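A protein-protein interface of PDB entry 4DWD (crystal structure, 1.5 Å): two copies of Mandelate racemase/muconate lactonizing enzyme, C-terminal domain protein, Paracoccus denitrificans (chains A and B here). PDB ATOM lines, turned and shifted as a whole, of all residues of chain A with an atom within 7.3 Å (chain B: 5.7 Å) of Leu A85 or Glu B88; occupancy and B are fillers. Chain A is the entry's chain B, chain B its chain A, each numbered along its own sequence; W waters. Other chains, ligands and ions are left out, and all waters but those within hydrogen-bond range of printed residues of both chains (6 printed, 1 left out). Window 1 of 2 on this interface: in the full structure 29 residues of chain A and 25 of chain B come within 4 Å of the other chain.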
ATOM      1  N   VAL A  54     -11.341  25.303  12.520  1.00  0.00           N
ATOM      2  CA  VAL A  54     -10.990  25.983  13.765  1.00  0.00           C
ATOM      3  C   VAL A  54     -11.726  27.323  13.851  1.00  0.00           C
ATOM      4  O   VAL A  54     -12.243  27.687  14.908  1.00  0.00           O
ATOM      5  CB  VAL A  54      -9.456  26.125  13.898  1.00  0.00           C
ATOM      6  CG1 VAL A  54      -9.095  27.085  15.023  1.00  0.00           C
ATOM      7  CG2 VAL A  54      -8.812  24.765  14.149  1.00  0.00           C
ATOM      8  N   ARG A  57     -15.588  26.294  14.583  1.00  0.00           N
ATOM      9  CA  ARG A  57     -15.878  25.648  15.866  1.00  0.00           C
ATOM     10  C   ARG A  57     -15.381  26.451  17.060  1.00  0.00           C
ATOM     11  O   ARG A  57     -16.038  26.495  18.103  1.00  0.00           O
ATOM     12  CB  ARG A  57     -15.234  24.263  15.938  1.00  0.00           C
ATOM     13  CG  ARG A  57     -15.829  23.184  15.054  1.00  0.00           C
ATOM     14  CD  ARG A  57     -15.258  21.821  15.440  1.00  0.00           C
ATOM     15  NE  ARG A  57     -13.791  21.790  15.378  1.00  0.00           N
ATOM     16  CZ  ARG A  57     -13.091  21.631  14.255  1.00  0.00           C
ATOM     17  NH1 ARG A  57     -13.710  21.464  13.091  1.00  0.00           N
ATOM     18  NH2 ARG A  57     -11.773  21.628  14.296  1.00  0.00           N
ATOM     19  N   ASP A  58     -14.204  27.051  16.918  1.00  0.00           N
ATOM     20  CA  ASP A  58     -13.497  27.604  18.073  1.00  0.00           C
ATOM     21  C   ASP A  58     -13.547  29.126  18.163  1.00  0.00           C
ATOM     22  O   ASP A  58     -13.734  29.682  19.256  1.00  0.00           O
ATOM     23  CB  ASP A  58     -12.048  27.105  18.118  1.00  0.00           C
ATOM     24  CG  ASP A  58     -11.941  25.589  18.062  1.00  0.00           C
ATOM     25  OD1 ASP A  58     -12.801  24.882  18.647  1.00  0.00           O
ATOM     26  OD2 ASP A  58     -10.992  25.088  17.433  1.00  0.00           O
ATOM     27  N   MET A  79      -5.833  33.273  20.795  1.00  0.00           N
ATOM     28  CA  MET A  79      -4.548  32.564  20.644  1.00  0.00           C
ATOM     29  C   MET A  79      -4.288  31.787  21.887  1.00  0.00           C
ATOM     30  O   MET A  79      -3.845  30.648  21.820  1.00  0.00           O
ATOM     31  CB  MET A  79      -3.303  33.450  20.319  1.00  0.00           C
ATOM     32  CG  MET A  79      -2.031  33.450  21.276  1.00  0.00           C
ATOM     33  SD  MET A  79      -1.147  31.678  21.500  1.00  0.00           S
ATOM     34  CE  MET A  79      -0.820  31.640  23.436  1.00  0.00           C
ATOM     35  N   ARG A  81      -6.495  30.632  24.097  1.00  0.00           N
ATOM     36  CA  ARG A  81      -7.457  29.510  24.139  1.00  0.00           C
ATOM     37  C   ARG A  81      -7.032  28.371  23.207  1.00  0.00           C
ATOM     38  O   ARG A  81      -7.267  27.191  23.500  1.00  0.00           O
ATOM     39  CB  ARG A  81      -8.863  29.966  23.741  1.00  0.00           C
ATOM     40  CG  ARG A  81      -9.442  31.047  24.637  1.00  0.00           C
ATOM     41  CD  ARG A  81     -10.886  30.796  25.042  1.00  0.00           C
ATOM     42  NE  ARG A  81     -11.756  30.383  23.947  1.00  0.00           N
ATOM     43  CZ  ARG A  81     -13.071  30.602  23.914  1.00  0.00           C
ATOM     44  NH1 ARG A  81     -13.789  30.184  22.879  1.00  0.00           N
ATOM     45  NH2 ARG A  81     -13.668  31.253  24.907  1.00  0.00           N
ATOM     46  N   LEU A  82      -6.415  28.736  22.086  1.00  0.00           N
ATOM     47  CA  LEU A  82      -6.066  27.776  21.043  1.00  0.00           C
ATOM     48  C   LEU A  82      -4.621  27.284  21.113  1.00  0.00           C
ATOM     49  O   LEU A  82      -4.170  26.541  20.236  1.00  0.00           O
ATOM     50  CB  LEU A  82      -6.298  28.392  19.660  1.00  0.00           C
ATOM     51  CG  LEU A  82      -7.708  28.794  19.249  1.00  0.00           C
ATOM     52  CD1 LEU A  82      -7.695  29.270  17.811  1.00  0.00           C
ATOM     53  CD2 LEU A  82      -8.657  27.626  19.438  1.00  0.00           C
ATOM     54  N   VAL A  83      -3.895  27.669  22.156  1.00  0.00           N
ATOM     55  CA  VAL A  83      -2.450  27.445  22.165  1.00  0.00           C
ATOM     56  C   VAL A  83      -2.100  25.960  22.051  1.00  0.00           C
ATOM     57  O   VAL A  83      -1.121  25.601  21.404  1.00  0.00           O
ATOM     58  CB  VAL A  83      -1.794  28.112  23.407  1.00  0.00           C
ATOM     59  CG1 VAL A  83      -2.250  27.445  24.698  1.00  0.00           C
ATOM     60  CG2 VAL A  83      -0.271  28.123  23.306  1.00  0.00           C
ATOM     61  N   LYS A  84      -2.926  25.093  22.637  1.00  0.00           N
ATOM     62  CA  LYS A  84      -2.620  23.661  22.637  1.00  0.00           C
ATOM     63  C   LYS A  84      -2.967  22.985  21.317  1.00  0.00           C
ATOM     64  O   LYS A  84      -2.764  21.784  21.178  1.00  0.00           O
ATOM     65  CB  LYS A  84      -3.286  22.945  23.820  1.00  0.00           C
ATOM     66  CG  LYS A  84      -2.979  23.521  25.203  1.00  0.00           C
ATOM     67  CD  LYS A  84      -1.824  22.774  25.840  1.00  0.00           C
ATOM     68  CE  LYS A  84      -1.608  23.159  27.294  1.00  0.00           C
ATOM     69  NZ  LYS A  84      -1.251  21.973  28.121  1.00  0.00           N
ATOM     70  N   LEU A  85      -3.446  23.770  20.345  1.00  0.00           N
ATOM     71  CA  LEU A  85      -3.579  23.302  18.959  1.00  0.00           C
ATOM     72  C   LEU A  85      -2.286  23.455  18.173  1.00  0.00           C
ATOM     73  O   LEU A  85      -2.226  23.104  16.993  1.00  0.00           O
ATOM     74  CB  LEU A  85      -4.739  24.004  18.226  1.00  0.00           C
ATOM     75  CG  LEU A  85      -6.135  23.834  18.830  1.00  0.00           C
ATOM     76  CD1 LEU A  85      -7.148  24.581  17.975  1.00  0.00           C
ATOM     77  CD2 LEU A  85      -6.501  22.356  18.978  1.00  0.00           C
ATOM     78  N   GLY A  86      -1.256  23.977  18.834  1.00  0.00           N
ATOM     79  CA  GLY A  86       0.055  24.139  18.233  1.00  0.00           C
ATOM     80  C   GLY A  86       0.731  25.357  18.842  1.00  0.00           C
ATOM     81  O   GLY A  86       1.566  25.221  19.728  1.00  0.00           O
ATOM     82  N   PRO A  87       0.351  26.562  18.394  1.00  0.00           N
ATOM     83  CA  PRO A  87      -0.694  26.887  17.419  1.00  0.00           C
ATOM     84  C   PRO A  87      -0.188  27.047  15.989  1.00  0.00           C
ATOM     85  O   PRO A  87      -0.958  27.461  15.102  1.00  0.00           O
ATOM     86  CB  PRO A  87      -1.240  28.205  17.954  1.00  0.00           C
ATOM     87  CG  PRO A  87      -0.008  28.879  18.498  1.00  0.00           C
ATOM     88  CD  PRO A  87       0.846  27.772  19.086  1.00  0.00           C
ATOM     89  N   GLU A  88       1.079  26.704  15.763  1.00  0.00           N
ATOM     90  CA  GLU A  88       1.712  26.898  14.454  1.00  0.00           C
ATOM     91  C   GLU A  88       0.895  26.293  13.328  1.00  0.00           C
ATOM     92  O   GLU A  88       0.433  25.151  13.413  1.00  0.00           O
ATOM     93  CB  GLU A  88       3.089  26.236  14.404  1.00  0.00           C
ATOM     94  CG  GLU A  88       4.156  26.855  15.302  1.00  0.00           C
ATOM     95  CD  GLU A  88       4.225  26.199  16.667  1.00  0.00           C
ATOM     96  OE1 GLU A  88       3.188  25.691  17.158  1.00  0.00           O
ATOM     97  OE2 GLU A  88       5.326  26.205  17.266  1.00  0.00           O
ATOM     98  N   GLY A  89       0.750  27.052  12.243  1.00  0.00           N
ATOM     99  CA  GLY A  89       0.140  26.517  11.022  1.00  0.00           C
ATOM    100  C   GLY A  89      -1.367  26.678  11.033  1.00  0.00           C
ATOM    101  O   GLY A  89      -1.887  27.756  10.777  1.00  0.00           O
ATOM    102  N   ILE A  90      -2.072  25.593  11.326  1.00  0.00           N
ATOM    103  CA  ILE A  90      -3.529  25.614  11.235  1.00  0.00           C
ATOM    104  C   ILE A  90      -4.175  26.725  12.076  1.00  0.00           C
ATOM    105  O   ILE A  90      -4.987  27.518  11.574  1.00  0.00           O
ATOM    106  CB  ILE A  90      -4.104  24.243  11.629  1.00  0.00           C
ATOM    107  CG1 ILE A  90      -3.780  23.210  10.535  1.00  0.00           C
ATOM    108  CG2 ILE A  90      -5.620  24.329  11.810  1.00  0.00           C
ATOM    109  CD1 ILE A  90      -3.908  21.766  10.982  1.00  0.00           C
ATOM    110  N   ALA A  91      -3.812  26.795  13.355  1.00  0.00           N
ATOM    111  CA  ALA A  91      -4.438  27.766  14.240  1.00  0.00           C
ATOM    112  C   ALA A  91      -3.969  29.192  13.968  1.00  0.00           C
ATOM    113  O   ALA A  91      -4.785  30.117  13.979  1.00  0.00           O
ATOM    114  CB  ALA A  91      -4.241  27.380  15.706  1.00  0.00           C
ATOM    115  N   THR A  92      -2.670  29.394  13.726  1.00  0.00           N
ATOM    116  CA  THR A  92      -2.232  30.753  13.420  1.00  0.00           C
ATOM    117  C   THR A  92      -2.840  31.283  12.116  1.00  0.00           C
ATOM    118  O   THR A  92      -3.107  32.477  12.024  1.00  0.00           O
ATOM    119  CB  THR A  92      -0.693  30.924  13.412  1.00  0.00           C
ATOM    120  OG1 THR A  92      -0.086  30.022  12.469  1.00  0.00           O
ATOM    121  CG2 THR A  92      -0.114  30.659  14.817  1.00  0.00           C
ATOM    122  N   HIS A 228      13.067  23.524   7.222  1.00  0.00           N
ATOM    123  CA  HIS A 228      12.725  24.673   8.067  1.00  0.00           C
ATOM    124  C   HIS A 228      12.821  24.356   9.533  1.00  0.00           C
ATOM    125  O   HIS A 228      13.027  25.255  10.340  1.00  0.00           O
ATOM    126  CB  HIS A 228      11.318  25.182   7.727  1.00  0.00           C
ATOM    127  CG  HIS A 228      10.230  24.509   8.520  1.00  0.00           C
ATOM    128  ND1 HIS A 228       9.757  23.286   8.213  1.00  0.00           N
ATOM    129  CD2 HIS A 228       9.554  24.919   9.664  1.00  0.00           C
ATOM    130  CE1 HIS A 228       8.830  22.924   9.117  1.00  0.00           C
ATOM    131  NE2 HIS A 228       8.707  23.926  10.009  1.00  0.00           N
ATOM    132  N   TYR A 229      12.657  23.074   9.873  1.00  0.00           N
ATOM    133  CA  TYR A 229      12.737  22.672  11.260  1.00  0.00           C
ATOM    134  C   TYR A 229      14.141  22.816  11.858  1.00  0.00           C
ATOM    135  O   TYR A 229      14.273  22.905  13.077  1.00  0.00           O
ATOM    136  CB  TYR A 229      12.127  21.275  11.489  1.00  0.00           C
ATOM    137  CG  TYR A 229      12.291  20.212  10.421  1.00  0.00           C
ATOM    138  CD1 TYR A 229      13.468  19.471  10.331  1.00  0.00           C
ATOM    139  CD2 TYR A 229      11.242  19.877   9.560  1.00  0.00           C
ATOM    140  CE1 TYR A 229      13.616  18.456   9.397  1.00  0.00           C
ATOM    141  CE2 TYR A 229      11.382  18.859   8.614  1.00  0.00           C
ATOM    142  CZ  TYR A 229      12.572  18.152   8.533  1.00  0.00           C
ATOM    143  OH  TYR A 229      12.725  17.136   7.602  1.00  0.00           O
ATOM    144  N   GLN A 250       7.765  29.482   6.911  1.00  0.00           N
ATOM    145  CA  GLN A 250       7.240  28.415   7.778  1.00  0.00           C
ATOM    146  C   GLN A 250       7.558  28.712   9.242  1.00  0.00           C
ATOM    147  O   GLN A 250       7.827  27.795  10.025  1.00  0.00           O
ATOM    148  CB  GLN A 250       7.807  27.060   7.382  1.00  0.00           C
ATOM    149  CG  GLN A 250       7.415  26.639   5.973  1.00  0.00           C
ATOM    150  CD  GLN A 250       7.912  25.247   5.645  1.00  0.00           C
ATOM    151  OE1 GLN A 250       7.376  24.247   6.126  1.00  0.00           O
ATOM    152  NE2 GLN A 250       8.950  25.170   4.822  1.00  0.00           N
ATOM    153  N   TYR A 252       5.754  30.793  12.490  1.00  0.00           N
ATOM    154  CA  TYR A 252       4.348  31.108  12.747  1.00  0.00           C
ATOM    155  C   TYR A 252       4.072  31.911  14.001  1.00  0.00           C
ATOM    156  O   TYR A 252       2.927  32.228  14.267  1.00  0.00           O
ATOM    157  CB  TYR A 252       3.497  29.823  12.762  1.00  0.00           C
ATOM    158  CG  TYR A 252       3.659  28.971  11.515  1.00  0.00           C
ATOM    159  CD1 TYR A 252       2.914  29.240  10.362  1.00  0.00           C
ATOM    160  CD2 TYR A 252       4.552  27.893  11.492  1.00  0.00           C
ATOM    161  CE1 TYR A 252       3.047  28.468   9.225  1.00  0.00           C
ATOM    162  CE2 TYR A 252       4.688  27.094  10.356  1.00  0.00           C
ATOM    163  CZ  TYR A 252       3.929  27.386   9.227  1.00  0.00           C
ATOM    164  OH  TYR A 252       4.047  26.643   8.065  1.00  0.00           O
ATOM    165  N   ALA A 256       9.129  32.553  17.663  1.00  0.00           N
ATOM    166  CA  ALA A 256       9.899  31.744  16.724  1.00  0.00           C
ATOM    167  C   ALA A 256      10.590  32.631  15.689  1.00  0.00           C
ATOM    168  O   ALA A 256      11.685  32.298  15.246  1.00  0.00           O
ATOM    169  CB  ALA A 256       9.036  30.674  16.041  1.00  0.00           C
ATOM    170  N   MET B  45      -7.257  18.145  22.595  1.00  0.00           N
ATOM    171  CA  MET B  45      -7.296  19.597  22.777  1.00  0.00           C
ATOM    172  C   MET B  45      -8.502  20.153  22.064  1.00  0.00           C
ATOM    173  O   MET B  45      -8.672  19.973  20.843  1.00  0.00           O
ATOM    174  CB  MET B  45      -5.983  20.191  22.278  1.00  0.00           C
ATOM    175  CG  MET B  45      -4.765  19.582  22.981  1.00  0.00           C
ATOM    176  SD  MET B  45      -4.717  19.883  24.925  1.00  0.00           S
ATOM    177  CE  MET B  45      -5.637  18.279  25.591  1.00  0.00           C
ATOM    178  N   LEU B  46      -9.365  20.814  22.832  1.00  0.00           N
ATOM    179  CA  LEU B  46     -10.673  21.262  22.333  1.00  0.00           C
ATOM    180  C   LEU B  46     -11.395  20.079  21.677  1.00  0.00           C
ATOM    181  O   LEU B  46     -12.046  20.220  20.639  1.00  0.00           O
ATOM    182  CB  LEU B  46     -10.521  22.476  21.392  1.00  0.00           C
ATOM    183  CG  LEU B  46      -9.982  23.764  22.029  1.00  0.00           C
ATOM    184  CD1 LEU B  46      -8.491  23.746  22.320  1.00  0.00           C
ATOM    185  CD2 LEU B  46     -10.288  24.941  21.124  1.00  0.00           C
ATOM    186  N   ALA B  50     -10.015  18.854  15.447  1.00  0.00           N
ATOM    187  CA  ALA B  50      -9.177  19.243  14.316  1.00  0.00           C
ATOM    188  C   ALA B  50      -8.206  18.118  13.921  1.00  0.00           C
ATOM    189  O   ALA B  50      -8.060  17.820  12.736  1.00  0.00           O
ATOM    190  CB  ALA B  50      -8.424  20.534  14.610  1.00  0.00           C
ATOM    191  N   LEU B  85       0.863  22.398   7.581  1.00  0.00           N
ATOM    192  CA  LEU B  85      -0.192  22.528   8.604  1.00  0.00           C
ATOM    193  C   LEU B  85       0.385  22.915   9.958  1.00  0.00           C
ATOM    194  O   LEU B  85      -0.352  23.044  10.935  1.00  0.00           O
ATOM    195  CB  LEU B  85      -0.985  21.216   8.737  1.00  0.00           C
ATOM    196  CG  LEU B  85      -1.737  20.789   7.471  1.00  0.00           C
ATOM    197  CD1 LEU B  85      -2.506  19.509   7.762  1.00  0.00           C
ATOM    198  CD2 LEU B  85      -2.673  21.878   6.945  1.00  0.00           C
ATOM    199  N   GLY B  86       1.700  23.103  10.005  1.00  0.00           N
ATOM    200  CA  GLY B  86       2.381  23.509  11.230  1.00  0.00           C
ATOM    201  C   GLY B  86       3.772  22.915  11.254  1.00  0.00           C
ATOM    202  O   GLY B  86       4.733  23.589  10.917  1.00  0.00           O
ATOM    203  N   PRO B  87       3.889  21.622  11.610  1.00  0.00           N
ATOM    204  CA  PRO B  87       2.805  20.684  11.910  1.00  0.00           C
ATOM    205  C   PRO B  87       2.478  20.584  13.399  1.00  0.00           C
ATOM    206  O   PRO B  87       1.684  19.719  13.806  1.00  0.00           O
ATOM    207  CB  PRO B  87       3.375  19.366  11.407  1.00  0.00           C
ATOM    208  CG  PRO B  87       4.828  19.482  11.767  1.00  0.00           C
ATOM    209  CD  PRO B  87       5.187  20.924  11.474  1.00  0.00           C
ATOM    210  N   GLU B  88       3.088  21.451  14.208  1.00  0.00           N
ATOM    211  CA  GLU B  88       2.935  21.386  15.675  1.00  0.00           C
ATOM    212  C   GLU B  88       1.490  21.364  16.114  1.00  0.00           C
ATOM    213  O   GLU B  88       0.673  22.159  15.639  1.00  0.00           O
ATOM    214  CB  GLU B  88       3.589  22.578  16.352  1.00  0.00           C
ATOM    215  CG  GLU B  88       5.100  22.656  16.198  1.00  0.00           C
ATOM    216  CD  GLU B  88       5.558  23.443  14.976  1.00  0.00           C
ATOM    217  OE1 GLU B  88       4.804  23.528  13.995  1.00  0.00           O
ATOM    218  OE2 GLU B  88       6.692  23.969  15.001  1.00  0.00           O
ATOM    219  N   GLY B  89       1.196  20.471  17.058  1.00  0.00           N
ATOM    220  CA  GLY B  89      -0.111  20.451  17.707  1.00  0.00           C
ATOM    221  C   GLY B  89      -1.063  19.540  16.948  1.00  0.00           C
ATOM    222  O   GLY B  89      -0.979  18.305  17.033  1.00  0.00           O
ATOM    223  N   ILE B  90      -1.978  20.156  16.206  1.00  0.00           N
ATOM    224  CA  ILE B  90      -3.012  19.400  15.497  1.00  0.00           C
ATOM    225  C   ILE B  90      -2.461  18.273  14.602  1.00  0.00           C
ATOM    226  O   ILE B  90      -2.891  17.126  14.709  1.00  0.00           O
ATOM    227  CB  ILE B  90      -3.924  20.342  14.684  1.00  0.00           C
ATOM    228  CG1 ILE B  90      -4.791  21.191  15.618  1.00  0.00           C
ATOM    229  CG2 ILE B  90      -4.838  19.555  13.756  1.00  0.00           C
ATOM    230  CD1 ILE B  90      -5.343  22.417  14.914  1.00  0.00           C
ATOM    231  N   ALA B  91      -1.501  18.595  13.735  1.00  0.00           N
ATOM    232  CA  ALA B  91      -1.005  17.597  12.786  1.00  0.00           C
ATOM    233  C   ALA B  91      -0.105  16.567  13.468  1.00  0.00           C
ATOM    234  O   ALA B  91      -0.214  15.373  13.190  1.00  0.00           O
ATOM    235  CB  ALA B  91      -0.310  18.263  11.608  1.00  0.00           C
ATOM    236  N   THR B  92       0.760  17.003  14.383  1.00  0.00           N
ATOM    237  CA  THR B  92       1.602  16.028  15.078  1.00  0.00           C
ATOM    238  C   THR B  92       0.790  15.061  15.950  1.00  0.00           C
ATOM    239  O   THR B  92       1.179  13.894  16.090  1.00  0.00           O
ATOM    240  CB  THR B  92       2.742  16.673  15.914  1.00  0.00           C
ATOM    241  OG1 THR B  92       2.206  17.556  16.901  1.00  0.00           O
ATOM    242  CG2 THR B  92       3.733  17.436  14.998  1.00  0.00           C
ATOM    243  N   TYR B 252       6.686  19.840  20.038  1.00  0.00           N
ATOM    244  CA  TYR B 252       5.999  18.905  19.145  1.00  0.00           C
ATOM    245  C   TYR B 252       6.854  18.281  18.063  1.00  0.00           C
ATOM    246  O   TYR B 252       6.356  17.483  17.282  1.00  0.00           O
ATOM    247  CB  TYR B 252       4.773  19.588  18.489  1.00  0.00           C
ATOM    248  CG  TYR B 252       3.807  20.200  19.486  1.00  0.00           C
ATOM    249  CD1 TYR B 252       2.833  19.422  20.110  1.00  0.00           C
ATOM    250  CD2 TYR B 252       3.873  21.566  19.816  1.00  0.00           C
ATOM    251  CE1 TYR B 252       1.948  19.975  21.025  1.00  0.00           C
ATOM    252  CE2 TYR B 252       2.989  22.130  20.742  1.00  0.00           C
ATOM    253  CZ  TYR B 252       2.018  21.323  21.335  1.00  0.00           C
ATOM    254  OH  TYR B 252       1.132  21.846  22.264  1.00  0.00           O
ATOM    255  N   THR B 253       8.126  18.663  17.988  1.00  0.00           N
ATOM    256  CA  THR B 253       9.042  18.034  17.027  1.00  0.00           C
ATOM    257  C   THR B 253      10.349  17.667  17.699  1.00  0.00           C
ATOM    258  O   THR B 253      10.722  18.237  18.734  1.00  0.00           O
ATOM    259  CB  THR B 253       9.364  18.955  15.827  1.00  0.00           C
ATOM    260  OG1 THR B 253      10.172  20.053  16.278  1.00  0.00           O
ATOM    261  CG2 THR B 253       8.069  19.463  15.147  1.00  0.00           C
HETATM  262  O   HOH W   1       5.669  24.533   8.254  1.00  0.00           O
HETATM  263  O   HOH W   2       1.283  24.447  22.635  1.00  0.00           O
HETATM  264  O   HOH W   3       7.067  24.209  12.294  1.00  0.00           O
HETATM  265  O   HOH W   4      -2.980  19.564  19.345  1.00  0.00           O
HETATM  266  O   HOH W   5      -1.259  19.930  22.575  1.00  0.00           O
HETATM  267  O   HOH W   6     -13.346  21.809  18.709  1.00  0.00           O
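Among the printed residues, pairs that only touch across the chains: Asp A58 with Leu B46 (3.5 Å), Arg A81 with Leu B46 (3.8 Å), Leu A82 with Leu B46 (3.6 Å), Lys A84 with Met B45 (3.5 Å), Leu A85 with Met B45 (3.7 Å), Leu A85 with Gly B89 (3.5 Å), Gly A86 with Glu B88 (3.3 Å), Gly A86 with Gly B89 (3.7 Å), Gly A86 with Tyr B252 (3.6 Å), Glu A88 with Gly B86 (3.4 Å), Gly A89 with Leu B85 (3.5 Å), Gly A89 with Gly B86 (3.8 Å), Ile A90 with Ile B90 (3.7 Å) and Tyr A252 with Gly B86 (3.5 Å).
Of the printed residues of chain B, Asp A58 touches Leu B46 (3.5 Å).
Pro A87 touches none of the printed residues of chain B.
Of the printed residues of chain B, Glu A88 touches Leu B85, Gly B86 and Glu B88.
Printed residues of chain B within 4 Å of Tyr A252: Gly B86 (3.5 Å).
Printed residues of chain A within 4 Å of Ala B50: Arg A57.
Of the printed residues of chain A, Gly B86 touches Glu A88 (3.4 Å), Gly A89 (3.8 Å) and Tyr A252 (3.5 Å).
Of chain A, only Leu A85 (3.3 Å), Gly A86 (3.3 Å) and Glu A88 (3.2 Å) come within 4 Å of Glu B88.
The nearest residue of chain A that does not touch Glu B88 is Pro A87 (5.0 Å).
Leu A85 touches Glu B88, and with the chains exchanged Glu A88 touches Leu B85.
Leu A85 touches Ile B90, and with the chains exchanged Ile A90 touches Leu B85.
Gly A86 touches Gly B89, and with the chains exchanged Gly A89 touches Gly B86.
Glu B88 touches its own counterpart, Glu A88.
Positions printed for both chains: 85, 86, 87, 88, 89, 90, 91, 92 and 252.
Water W2 lies within hydrogen-bond range of OH of Tyr B252 (2.6 Å), O of Val A83 (2.9 Å) and O of Gly A86 (3.0 Å).
Water W1 lies within hydrogen-bond range of OH of Tyr A252, OE1 of Gln A250 and O of Gly B86.
Water W3 lies within hydrogen-bond range of the side-chain carboxylate (OE2) of Glu B88 (2.7 Å), the backbone carbonyl oxygen (O) of Gly B86 (2.8 Å) and a ring nitrogen (NE2) of His A228 (2.8 Å).
Water W5 lies within hydrogen-bond range of O of Lys A84 (2.8 Å) and OH of Tyr B252 (3.1 Å).
Water W6 lies within hydrogen-bond range of O of Leu B46, OD1 of Asp A58 and NE of Arg A57.
Water W4 lies within hydrogen-bond range of O of Lys A84 (2.9 Å), O of Gly B89 (3.3 Å) and N of Ile B90 (3.3 Å).
Of the 13 printed residues of chain B, 9 touch a printed residue of chain A.
Hydrophobic or aromatic side chains of chain B within 4 Å of the printed part of chain A: Met B45, Leu B46, Ala B50, Leu B85, Ile B90 and Tyr B252.
Of the 21 printed residues of chain A, 11 touch a printed residue of chain B.
Hydrophobic or aromatic side chains of chain A within 4 Å of the printed part of chain B: Leu A82, Leu A85, Ile A90 and Tyr A252.
Among the printed residues, 20 pairs touch across the chains.
Among the printed residues, no Asp or Glu carboxylate lies within 4 Å of a Lys or Arg side-chain nitrogen of the other chain.
The guanidinium group (NH2) of Arg A57 lies close to the backbone NH (N) of Ala B50, at 3.5 Å.
N of Ile B90 is in hydrogen-bond range of O of Leu A85.
The backbone carbonyl oxygen (O) of Leu B85 lies within hydrogen-bond range of the backbone NH (N) of Ile A90, at 3.1 Å.
The backbone carbonyl oxygen of Leu A85 sits close to the backbone carbonyl oxygen of Glu B88, at 3.3 Å.
O of Leu B85 sits close to O of Glu A88 (3.3 Å).
The side-chain carboxylate (OE2) of Glu B88 lies close to the side-chain carboxylate (OE2) of Glu A88 (3.5 Å).
N of Gly B89 is in hydrogen-bond range of OG1 of Thr B92 (3.1 Å).
The backbone NH (N) of Gly A89 lies within hydrogen-bond range of the side-chain hydroxyl (OG1) of Thr A92 (3.1 Å).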
